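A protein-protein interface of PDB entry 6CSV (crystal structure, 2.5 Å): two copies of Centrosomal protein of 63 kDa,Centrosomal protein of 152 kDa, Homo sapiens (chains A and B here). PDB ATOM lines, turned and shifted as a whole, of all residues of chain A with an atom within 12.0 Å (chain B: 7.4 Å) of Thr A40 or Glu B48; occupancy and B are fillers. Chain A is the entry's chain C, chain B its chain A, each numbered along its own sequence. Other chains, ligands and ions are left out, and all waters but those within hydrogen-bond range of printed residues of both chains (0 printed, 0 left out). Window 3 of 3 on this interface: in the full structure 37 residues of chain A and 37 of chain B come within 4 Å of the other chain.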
ATOM      1  N   GLU A  31      -5.224  -8.108   6.563  1.00  0.00           N
ATOM      2  CA  GLU A  31      -5.027  -8.005   7.992  1.00  0.00           C
ATOM      3  C   GLU A  31      -4.001  -9.015   8.526  1.00  0.00           C
ATOM      4  O   GLU A  31      -3.241  -8.703   9.417  1.00  0.00           O
ATOM      5  CB  GLU A  31      -6.344  -8.161   8.741  1.00  0.00           C
ATOM      6  CG  GLU A  31      -7.252  -6.947   8.665  1.00  0.00           C
ATOM      7  CD  GLU A  31      -8.450  -7.054   9.614  1.00  0.00           C
ATOM      8  OE1 GLU A  31      -9.130  -8.125   9.659  1.00  0.00           O
ATOM      9  OE2 GLU A  31      -8.709  -6.043  10.314  1.00  0.00           O
ATOM     10  N   SER A  32      -3.959 -10.208   7.977  1.00  0.00           N
ATOM     11  CA  SER A  32      -3.079 -11.220   8.517  1.00  0.00           C
ATOM     12  C   SER A  32      -1.603 -11.036   8.115  1.00  0.00           C
ATOM     13  O   SER A  32      -0.710 -11.334   8.918  1.00  0.00           O
ATOM     14  CB  SER A  32      -3.607 -12.611   8.170  1.00  0.00           C
ATOM     15  OG  SER A  32      -3.541 -12.857   6.783  1.00  0.00           O
ATOM     16  N   GLU A  33      -1.332 -10.550   6.895  1.00  0.00           N
ATOM     17  CA  GLU A  33       0.035 -10.144   6.522  1.00  0.00           C
ATOM     18  C   GLU A  33       0.527  -9.003   7.435  1.00  0.00           C
ATOM     19  O   GLU A  33       1.641  -9.043   7.940  1.00  0.00           O
ATOM     20  CB  GLU A  33       0.188  -9.789   5.016  1.00  0.00           C
ATOM     21  CG  GLU A  33      -0.613  -8.590   4.468  1.00  0.00           C
ATOM     22  CD  GLU A  33      -0.220  -8.135   3.037  1.00  0.00           C
ATOM     23  OE1 GLU A  33       0.812  -8.616   2.480  1.00  0.00           O
ATOM     24  OE2 GLU A  33      -0.956  -7.263   2.475  1.00  0.00           O
ATOM     25  N   LYS A  34      -0.314  -8.012   7.689  1.00  0.00           N
ATOM     26  CA  LYS A  34       0.056  -6.942   8.603  1.00  0.00           C
ATOM     27  C   LYS A  34       0.496  -7.519   9.964  1.00  0.00           C
ATOM     28  O   LYS A  34       1.597  -7.267  10.436  1.00  0.00           O
ATOM     29  CB  LYS A  34      -1.105  -5.972   8.739  1.00  0.00           C
ATOM     30  CG  LYS A  34      -0.935  -4.887   9.788  1.00  0.00           C
ATOM     31  CD  LYS A  34      -2.252  -4.185  10.112  1.00  0.00           C
ATOM     32  CE  LYS A  34      -2.995  -3.602   8.906  1.00  0.00           C
ATOM     33  NZ  LYS A  34      -4.333  -3.095   9.324  1.00  0.00           N
ATOM     34  N   THR A  35      -0.356  -8.340  10.547  1.00  0.00           N
ATOM     35  CA  THR A  35      -0.110  -8.928  11.849  1.00  0.00           C
ATOM     36  C   THR A  35       1.105  -9.844  11.865  1.00  0.00           C
ATOM     37  O   THR A  35       1.828  -9.871  12.860  1.00  0.00           O
ATOM     38  CB  THR A  35      -1.385  -9.660  12.356  1.00  0.00           C
ATOM     39  OG1 THR A  35      -2.380  -8.681  12.677  1.00  0.00           O
ATOM     40  CG2 THR A  35      -1.131 -10.507  13.600  1.00  0.00           C
ATOM     41  N   VAL A  36       1.335 -10.596  10.799  1.00  0.00           N
ATOM     42  CA  VAL A  36       2.535 -11.427  10.756  1.00  0.00           C
ATOM     43  C   VAL A  36       3.787 -10.533  10.647  1.00  0.00           C
ATOM     44  O   VAL A  36       4.865 -10.885  11.174  1.00  0.00           O
ATOM     45  CB  VAL A  36       2.481 -12.504   9.646  1.00  0.00           C
ATOM     46  CG1 VAL A  36       3.812 -13.249   9.501  1.00  0.00           C
ATOM     47  CG2 VAL A  36       1.398 -13.520   9.965  1.00  0.00           C
ATOM     48  N   ARG A  37       3.646  -9.381   9.995  1.00  0.00           N
ATOM     49  CA  ARG A  37       4.750  -8.426   9.921  1.00  0.00           C
ATOM     50  C   ARG A  37       5.090  -7.783  11.274  1.00  0.00           C
ATOM     51  O   ARG A  37       6.264  -7.669  11.617  1.00  0.00           O
ATOM     52  CB  ARG A  37       4.518  -7.368   8.832  1.00  0.00           C
ATOM     53  CG  ARG A  37       5.260  -7.705   7.543  1.00  0.00           C
ATOM     54  CD  ARG A  37       5.277  -6.535   6.574  1.00  0.00           C
ATOM     55  NE  ARG A  37       3.921  -6.188   6.133  1.00  0.00           N
ATOM     56  CZ  ARG A  37       3.179  -5.175   6.589  1.00  0.00           C
ATOM     57  NH1 ARG A  37       3.635  -4.332   7.517  1.00  0.00           N
ATOM     58  NH2 ARG A  37       1.962  -4.987   6.083  1.00  0.00           N
ATOM     59  N   GLN A  38       4.070  -7.390  12.033  1.00  0.00           N
ATOM     60  CA  GLN A  38       4.239  -6.911  13.417  1.00  0.00           C
ATOM     61  C   GLN A  38       5.101  -7.895  14.232  1.00  0.00           C
ATOM     62  O   GLN A  38       6.165  -7.525  14.712  1.00  0.00           O
ATOM     63  CB  GLN A  38       2.862  -6.702  14.074  1.00  0.00           C
ATOM     64  CG  GLN A  38       2.821  -5.810  15.303  1.00  0.00           C
ATOM     65  CD  GLN A  38       1.421  -5.260  15.571  1.00  0.00           C
ATOM     66  OE1 GLN A  38       0.419  -5.941  15.348  1.00  0.00           O
ATOM     67  NE2 GLN A  38       1.349  -4.013  16.045  1.00  0.00           N
ATOM     68  N   PHE A  39       4.667  -9.149  14.320  1.00  0.00           N
ATOM     69  CA  PHE A  39       5.401 -10.192  15.060  1.00  0.00           C
ATOM     70  C   PHE A  39       6.832 -10.448  14.556  1.00  0.00           C
ATOM     71  O   PHE A  39       7.714 -10.688  15.363  1.00  0.00           O
ATOM     72  CB  PHE A  39       4.613 -11.527  15.088  1.00  0.00           C
ATOM     73  CG  PHE A  39       5.300 -12.625  15.859  1.00  0.00           C
ATOM     74  CD1 PHE A  39       5.134 -12.737  17.230  1.00  0.00           C
ATOM     75  CD2 PHE A  39       6.118 -13.544  15.206  1.00  0.00           C
ATOM     76  CE1 PHE A  39       5.774 -13.748  17.943  1.00  0.00           C
ATOM     77  CE2 PHE A  39       6.766 -14.554  15.901  1.00  0.00           C
ATOM     78  CZ  PHE A  39       6.600 -14.656  17.276  1.00  0.00           C
ATOM     79  N   THR A  40       7.059 -10.394  13.244  1.00  0.00           N
ATOM     80  CA  THR A  40       8.401 -10.611  12.669  1.00  0.00           C
ATOM     81  C   THR A  40       9.319  -9.424  12.917  1.00  0.00           C
ATOM     82  O   THR A  40      10.518  -9.612  13.092  1.00  0.00           O
ATOM     83  CB  THR A  40       8.323 -10.923  11.162  1.00  0.00           C
ATOM     84  OG1 THR A  40       7.676 -12.185  10.995  1.00  0.00           O
ATOM     85  CG2 THR A  40       9.706 -10.982  10.503  1.00  0.00           C
ATOM     86  N   ALA A  41       8.755  -8.213  12.934  1.00  0.00           N
ATOM     87  CA  ALA A  41       9.496  -7.012  13.331  1.00  0.00           C
ATOM     88  C   ALA A  41       9.706  -6.932  14.847  1.00  0.00           C
ATOM     89  O   ALA A  41      10.458  -6.074  15.305  1.00  0.00           O
ATOM     90  CB  ALA A  41       8.805  -5.752  12.826  1.00  0.00           C
ATOM     91  N   LEU A  42       9.030  -7.788  15.619  1.00  0.00           N
ATOM     92  CA  LEU A  42       9.291  -7.971  17.065  1.00  0.00           C
ATOM     93  C   LEU A  42      10.043  -9.309  17.352  1.00  0.00           C
ATOM     94  O   LEU A  42      10.599  -9.930  16.436  1.00  0.00           O
ATOM     95  CB  LEU A  42       7.961  -7.845  17.838  1.00  0.00           C
ATOM     96  CG  LEU A  42       7.477  -6.444  18.271  1.00  0.00           C
ATOM     97  CD1 LEU A  42       7.856  -5.329  17.300  1.00  0.00           C
ATOM     98  CD2 LEU A  42       5.968  -6.456  18.503  1.00  0.00           C
ATOM     99  N   LYS A  43      10.106  -9.712  18.624  1.00  0.00           N
ATOM    100  CA  LYS A  43      10.749 -10.974  19.039  1.00  0.00           C
ATOM    101  C   LYS A  43       9.805 -11.814  19.901  1.00  0.00           C
ATOM    102  O   LYS A  43       8.822 -12.366  19.397  1.00  0.00           O
ATOM    103  CB  LYS A  43      12.089 -10.712  19.761  1.00  0.00           C
ATOM    104  CG  LYS A  43      12.079  -9.686  20.892  1.00  0.00           C
ATOM    105  CD  LYS A  43      13.297  -8.773  20.830  1.00  0.00           C
ATOM    106  CE  LYS A  43      13.147  -7.671  19.785  1.00  0.00           C
ATOM    107  NZ  LYS A  43      12.473  -6.452  20.340  1.00  0.00           N
ATOM    108  N   GLY A  49      -0.152 -12.955  21.594  1.00  0.00           N
ATOM    109  CA  GLY A  49      -0.947 -11.769  21.279  1.00  0.00           C
ATOM    110  C   GLY A  49      -1.237 -11.672  19.788  1.00  0.00           C
ATOM    111  O   GLY A  49      -2.350 -11.335  19.379  1.00  0.00           O
ATOM    112  N   ALA A  50      -0.226 -11.952  18.973  1.00  0.00           N
ATOM    113  CA  ALA A  50      -0.396 -12.074  17.527  1.00  0.00           C
ATOM    114  C   ALA A  50      -1.282 -13.272  17.149  1.00  0.00           C
ATOM    115  O   ALA A  50      -1.952 -13.207  16.112  1.00  0.00           O
ATOM    116  CB  ALA A  50       0.955 -12.183  16.835  1.00  0.00           C
ATOM    117  N   LEU A  51      -1.278 -14.337  17.974  1.00  0.00           N
ATOM    118  CA  LEU A  51      -2.163 -15.508  17.795  1.00  0.00           C
ATOM    119  C   LEU A  51      -3.642 -15.162  17.915  1.00  0.00           C
ATOM    120  O   LEU A  51      -4.470 -15.804  17.271  1.00  0.00           O
ATOM    121  CB  LEU A  51      -1.823 -16.687  18.752  1.00  0.00           C
ATOM    122  CG  LEU A  51      -1.720 -16.667  20.316  1.00  0.00           C
ATOM    123  CD1 LEU A  51      -0.305 -16.411  20.861  1.00  0.00           C
ATOM    124  CD2 LEU A  51      -2.724 -15.763  21.044  1.00  0.00           C
ATOM    125  N   GLU A  53      -4.906 -11.971  17.290  1.00  0.00           N
ATOM    126  CA  GLU A  53      -5.296 -11.100  16.193  1.00  0.00           C
ATOM    127  C   GLU A  53      -5.654 -11.950  14.971  1.00  0.00           C
ATOM    128  O   GLU A  53      -6.717 -11.791  14.397  1.00  0.00           O
ATOM    129  CB  GLU A  53      -4.180 -10.121  15.849  1.00  0.00           C
ATOM    130  CG  GLU A  53      -4.052  -8.919  16.770  1.00  0.00           C
ATOM    131  CD  GLU A  53      -3.396  -7.745  16.063  1.00  0.00           C
ATOM    132  OE1 GLU A  53      -2.568  -7.978  15.150  1.00  0.00           O
ATOM    133  OE2 GLU A  53      -3.714  -6.587  16.408  1.00  0.00           O
ATOM    134  N   LEU A  54      -4.751 -12.872  14.640  1.00  0.00           N
ATOM    135  CA  LEU A  54      -4.853 -13.770  13.502  1.00  0.00           C
ATOM    136  C   LEU A  54      -6.088 -14.656  13.561  1.00  0.00           C
ATOM    137  O   LEU A  54      -6.872 -14.724  12.601  1.00  0.00           O
ATOM    138  CB  LEU A  54      -3.620 -14.655  13.459  1.00  0.00           C
ATOM    139  CG  LEU A  54      -3.311 -15.305  12.134  1.00  0.00           C
ATOM    140  CD1 LEU A  54      -3.028 -14.246  11.075  1.00  0.00           C
ATOM    141  CD2 LEU A  54      -2.128 -16.256  12.304  1.00  0.00           C
ATOM    142  N   PHE B  39       3.397 -23.291  17.456  1.00  0.00           N
ATOM    143  CA  PHE B  39       3.801 -21.876  17.578  1.00  0.00           C
ATOM    144  C   PHE B  39       3.901 -21.355  19.023  1.00  0.00           C
ATOM    145  O   PHE B  39       4.780 -20.533  19.308  1.00  0.00           O
ATOM    146  CB  PHE B  39       2.858 -20.969  16.770  1.00  0.00           C
ATOM    147  CG  PHE B  39       2.851 -19.538  17.235  1.00  0.00           C
ATOM    148  CD1 PHE B  39       3.945 -18.712  16.993  1.00  0.00           C
ATOM    149  CD2 PHE B  39       1.762 -19.019  17.935  1.00  0.00           C
ATOM    150  CE1 PHE B  39       3.958 -17.394  17.433  1.00  0.00           C
ATOM    151  CE2 PHE B  39       1.772 -17.705  18.371  1.00  0.00           C
ATOM    152  CZ  PHE B  39       2.867 -16.889  18.122  1.00  0.00           C
ATOM    153  N   LEU B  42       7.389 -22.580  20.439  1.00  0.00           N
ATOM    154  CA  LEU B  42       8.598 -21.977  19.878  1.00  0.00           C
ATOM    155  C   LEU B  42       8.834 -20.509  20.295  1.00  0.00           C
ATOM    156  O   LEU B  42       9.809 -19.917  19.825  1.00  0.00           O
ATOM    157  CB  LEU B  42       8.596 -22.100  18.335  1.00  0.00           C
ATOM    158  CG  LEU B  42       8.309 -23.491  17.741  1.00  0.00           C
ATOM    159  CD1 LEU B  42       8.322 -23.510  16.216  1.00  0.00           C
ATOM    160  CD2 LEU B  42       9.307 -24.488  18.295  1.00  0.00           C
ATOM    161  N   LYS B  43       7.970 -19.943  21.163  1.00  0.00           N
ATOM    162  CA  LYS B  43       8.067 -18.555  21.673  1.00  0.00           C
ATOM    163  C   LYS B  43       7.712 -17.575  20.549  1.00  0.00           C
ATOM    164  O   LYS B  43       7.543 -16.371  20.768  1.00  0.00           O
ATOM    165  CB  LYS B  43       9.449 -18.208  22.309  1.00  0.00           C
ATOM    166  CG  LYS B  43       9.700 -18.707  23.739  1.00  0.00           C
ATOM    167  CD  LYS B  43      10.279 -20.116  23.807  1.00  0.00           C
ATOM    168  CE  LYS B  43      11.745 -20.188  23.396  1.00  0.00           C
ATOM    169  NZ  LYS B  43      12.107 -21.561  22.942  1.00  0.00           N
ATOM    170  N   GLY B  46      12.067 -20.527  14.744  1.00  0.00           N
ATOM    171  CA  GLY B  46      11.161 -20.727  13.618  1.00  0.00           C
ATOM    172  C   GLY B  46       9.725 -20.269  13.867  1.00  0.00           C
ATOM    173  O   GLY B  46       8.813 -20.664  13.136  1.00  0.00           O
ATOM    174  N   SER B  47       9.529 -19.407  14.870  1.00  0.00           N
ATOM    175  CA  SER B  47       8.192 -19.061  15.382  1.00  0.00           C
ATOM    176  C   SER B  47       7.346 -18.379  14.321  1.00  0.00           C
ATOM    177  O   SER B  47       6.127 -18.522  14.299  1.00  0.00           O
ATOM    178  CB  SER B  47       8.313 -18.128  16.589  1.00  0.00           C
ATOM    179  OG  SER B  47       7.260 -18.357  17.495  1.00  0.00           O
ATOM    180  N   GLU B  48       8.017 -17.644  13.444  1.00  0.00           N
ATOM    181  CA  GLU B  48       7.390 -16.804  12.456  1.00  0.00           C
ATOM    182  C   GLU B  48       7.009 -17.599  11.204  1.00  0.00           C
ATOM    183  O   GLU B  48       5.902 -17.456  10.699  1.00  0.00           O
ATOM    184  CB  GLU B  48       8.329 -15.623  12.134  1.00  0.00           C
ATOM    185  CG  GLU B  48       9.543 -15.936  11.239  1.00  0.00           C
ATOM    186  CD  GLU B  48      10.631 -14.893  11.338  1.00  0.00           C
ATOM    187  OE1 GLU B  48      11.308 -14.878  12.387  1.00  0.00           O
ATOM    188  OE2 GLU B  48      10.802 -14.094  10.384  1.00  0.00           O
ATOM    189  N   GLY B  49       7.906 -18.461  10.724  1.00  0.00           N
ATOM    190  CA  GLY B  49       7.605 -19.373   9.613  1.00  0.00           C
ATOM    191  C   GLY B  49       6.407 -20.242   9.943  1.00  0.00           C
ATOM    192  O   GLY B  49       5.580 -20.517   9.075  1.00  0.00           O
ATOM    193  N   ALA B  50       6.326 -20.636  11.216  1.00  0.00           N
ATOM    194  CA  ALA B  50       5.166 -21.305  11.817  1.00  0.00           C
ATOM    195  C   ALA B  50       3.915 -20.420  12.026  1.00  0.00           C
ATOM    196  O   ALA B  50       2.798 -20.916  12.023  1.00  0.00           O
ATOM    197  CB  ALA B  50       5.587 -21.923  13.153  1.00  0.00           C
ATOM    198  N   LEU B  51       4.095 -19.132  12.282  1.00  0.00           N
ATOM    199  CA  LEU B  51       2.959 -18.187  12.266  1.00  0.00           C
ATOM    200  C   LEU B  51       2.427 -17.912  10.833  1.00  0.00           C
ATOM    201  O   LEU B  51       1.234 -17.660  10.658  1.00  0.00           O
ATOM    202  CB  LEU B  51       3.332 -16.872  12.957  1.00  0.00           C
ATOM    203  CG  LEU B  51       2.184 -15.895  13.231  1.00  0.00           C
ATOM    204  CD1 LEU B  51       1.402 -16.325  14.454  1.00  0.00           C
ATOM    205  CD2 LEU B  51       2.694 -14.483  13.427  1.00  0.00           C
ATOM    206  N   GLU B  52       3.303 -17.932   9.827  1.00  0.00           N
ATOM    207  CA  GLU B  52       2.858 -17.823   8.433  1.00  0.00           C
ATOM    208  C   GLU B  52       2.060 -19.029   8.024  1.00  0.00           C
ATOM    209  O   GLU B  52       1.050 -18.885   7.323  1.00  0.00           O
ATOM    210  CB  GLU B  52       4.017 -17.639   7.430  1.00  0.00           C
ATOM    211  CG  GLU B  52       4.075 -16.275   6.734  1.00  0.00           C
ATOM    212  CD  GLU B  52       2.773 -15.851   6.043  1.00  0.00           C
ATOM    213  OE1 GLU B  52       1.955 -16.707   5.634  1.00  0.00           O
ATOM    214  OE2 GLU B  52       2.567 -14.623   5.902  1.00  0.00           O
ATOM    215  N   GLU B  53       2.525 -20.215   8.432  1.00  0.00           N
ATOM    216  CA  GLU B  53       1.824 -21.479   8.142  1.00  0.00           C
ATOM    217  C   GLU B  53       0.403 -21.512   8.714  1.00  0.00           C
ATOM    218  O   GLU B  53      -0.528 -21.944   8.036  1.00  0.00           O
ATOM    219  CB  GLU B  53       2.625 -22.681   8.643  1.00  0.00           C
ATOM    220  CG  GLU B  53       3.772 -23.092   7.726  1.00  0.00           C
ATOM    221  CD  GLU B  53       4.425 -24.399   8.161  1.00  0.00           C
ATOM    222  OE1 GLU B  53       3.979 -24.998   9.166  1.00  0.00           O
ATOM    223  OE2 GLU B  53       5.395 -24.832   7.498  1.00  0.00           O
ATOM    224  N   LEU B  54       0.246 -21.047   9.944  1.00  0.00           N
ATOM    225  CA  LEU B  54      -1.076 -20.874  10.539  1.00  0.00           C
ATOM    226  C   LEU B  54      -1.933 -19.922   9.726  1.00  0.00           C
ATOM    227  O   LEU B  54      -3.095 -20.210   9.446  1.00  0.00           O
ATOM    228  CB  LEU B  54      -0.979 -20.302  11.960  1.00  0.00           C
ATOM    229  CG  LEU B  54      -2.298 -20.088  12.717  1.00  0.00           C
ATOM    230  CD1 LEU B  54      -3.063 -21.401  12.862  1.00  0.00           C
ATOM    231  CD2 LEU B  54      -2.047 -19.462  14.080  1.00  0.00           C
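O of Val A36 lies within hydrogen-bond range of OG1 of Thr A40 (3.1 Å).
Of chain B, only Glu B48 comes within 4 Å of Thr A40.
Glu B48 touches one residue of chain A.
Gly B49 touches none of the printed residues of chain A.
No residue of chain A comes within 4 Å of Ala B50.
Glu B52 touches none of the printed residues of chain A.
Printed residues of chain A within 4 Å of Leu B51: Val A36, Phe A39 and Leu A54.
Of the printed residues of chain B, Phe A39 touches Phe B39 (3.8 Å), Ser B47 (3.8 Å) and Leu B51 (3.9 Å).
Of the printed residues of chain B, Val A36 touches Leu B51.
Of the printed residues of chain B, Leu A51 touches Phe B39.
Leu A42 touches none of the printed residues of chain B.
Arg A37 touches none of the printed residues of chain B.
The nearest residue of chain B that does not touch Thr A40 is Leu B51 (6.0 Å).
The nearest residue of chain A that does not touch Glu B48 is Phe A39 (4.1 Å).
Among the printed residues, pairs that only touch across the chains: Thr A40 with Glu B48 (3.3 Å), Leu A51 with Phe B39 (3.5 Å), Leu A54 with Leu B54 (3.7 Å), Phe A39 with Ser B47 (3.8 Å), Phe A39 with Phe B39 (3.8 Å), Val A36 with Leu B51 (3.8 Å), Phe A39 with Leu B51 (3.9 Å) and Leu A54 with Leu B51 (3.998 Å).
Hydrophobic or aromatic side chains of chain B within 4 Å of the printed part of chain A: Phe B39, Leu B51 and Leu B54.
Printed residues of chain A that touch a printed residue of chain B: Val A36, Phe A39, Thr A40, Leu A51 and Leu A54.
Hydrophobic or aromatic side chains of chain A within 4 Å of the printed part of chain B: Val A36, Phe A39, Leu A51 and Leu A54.
Phe A39 touches its own counterpart, Phe B39.
Phe A39 touches Leu B51, and with the chains exchanged Leu A51 touches Phe B39.
Leu A54 touches Leu B51, but with the chains exchanged Leu A51 does not touch Leu B54 (5.4 Å).
Leu A54 touches its own counterpart, Leu B54.
Positions printed for both chains: 39, 42, 43, 49, 50, 51, 53 and 54.
Of the 8 pairs that touch across the chains among the printed residues, 4 have their exchanged pair printed and touching as well.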
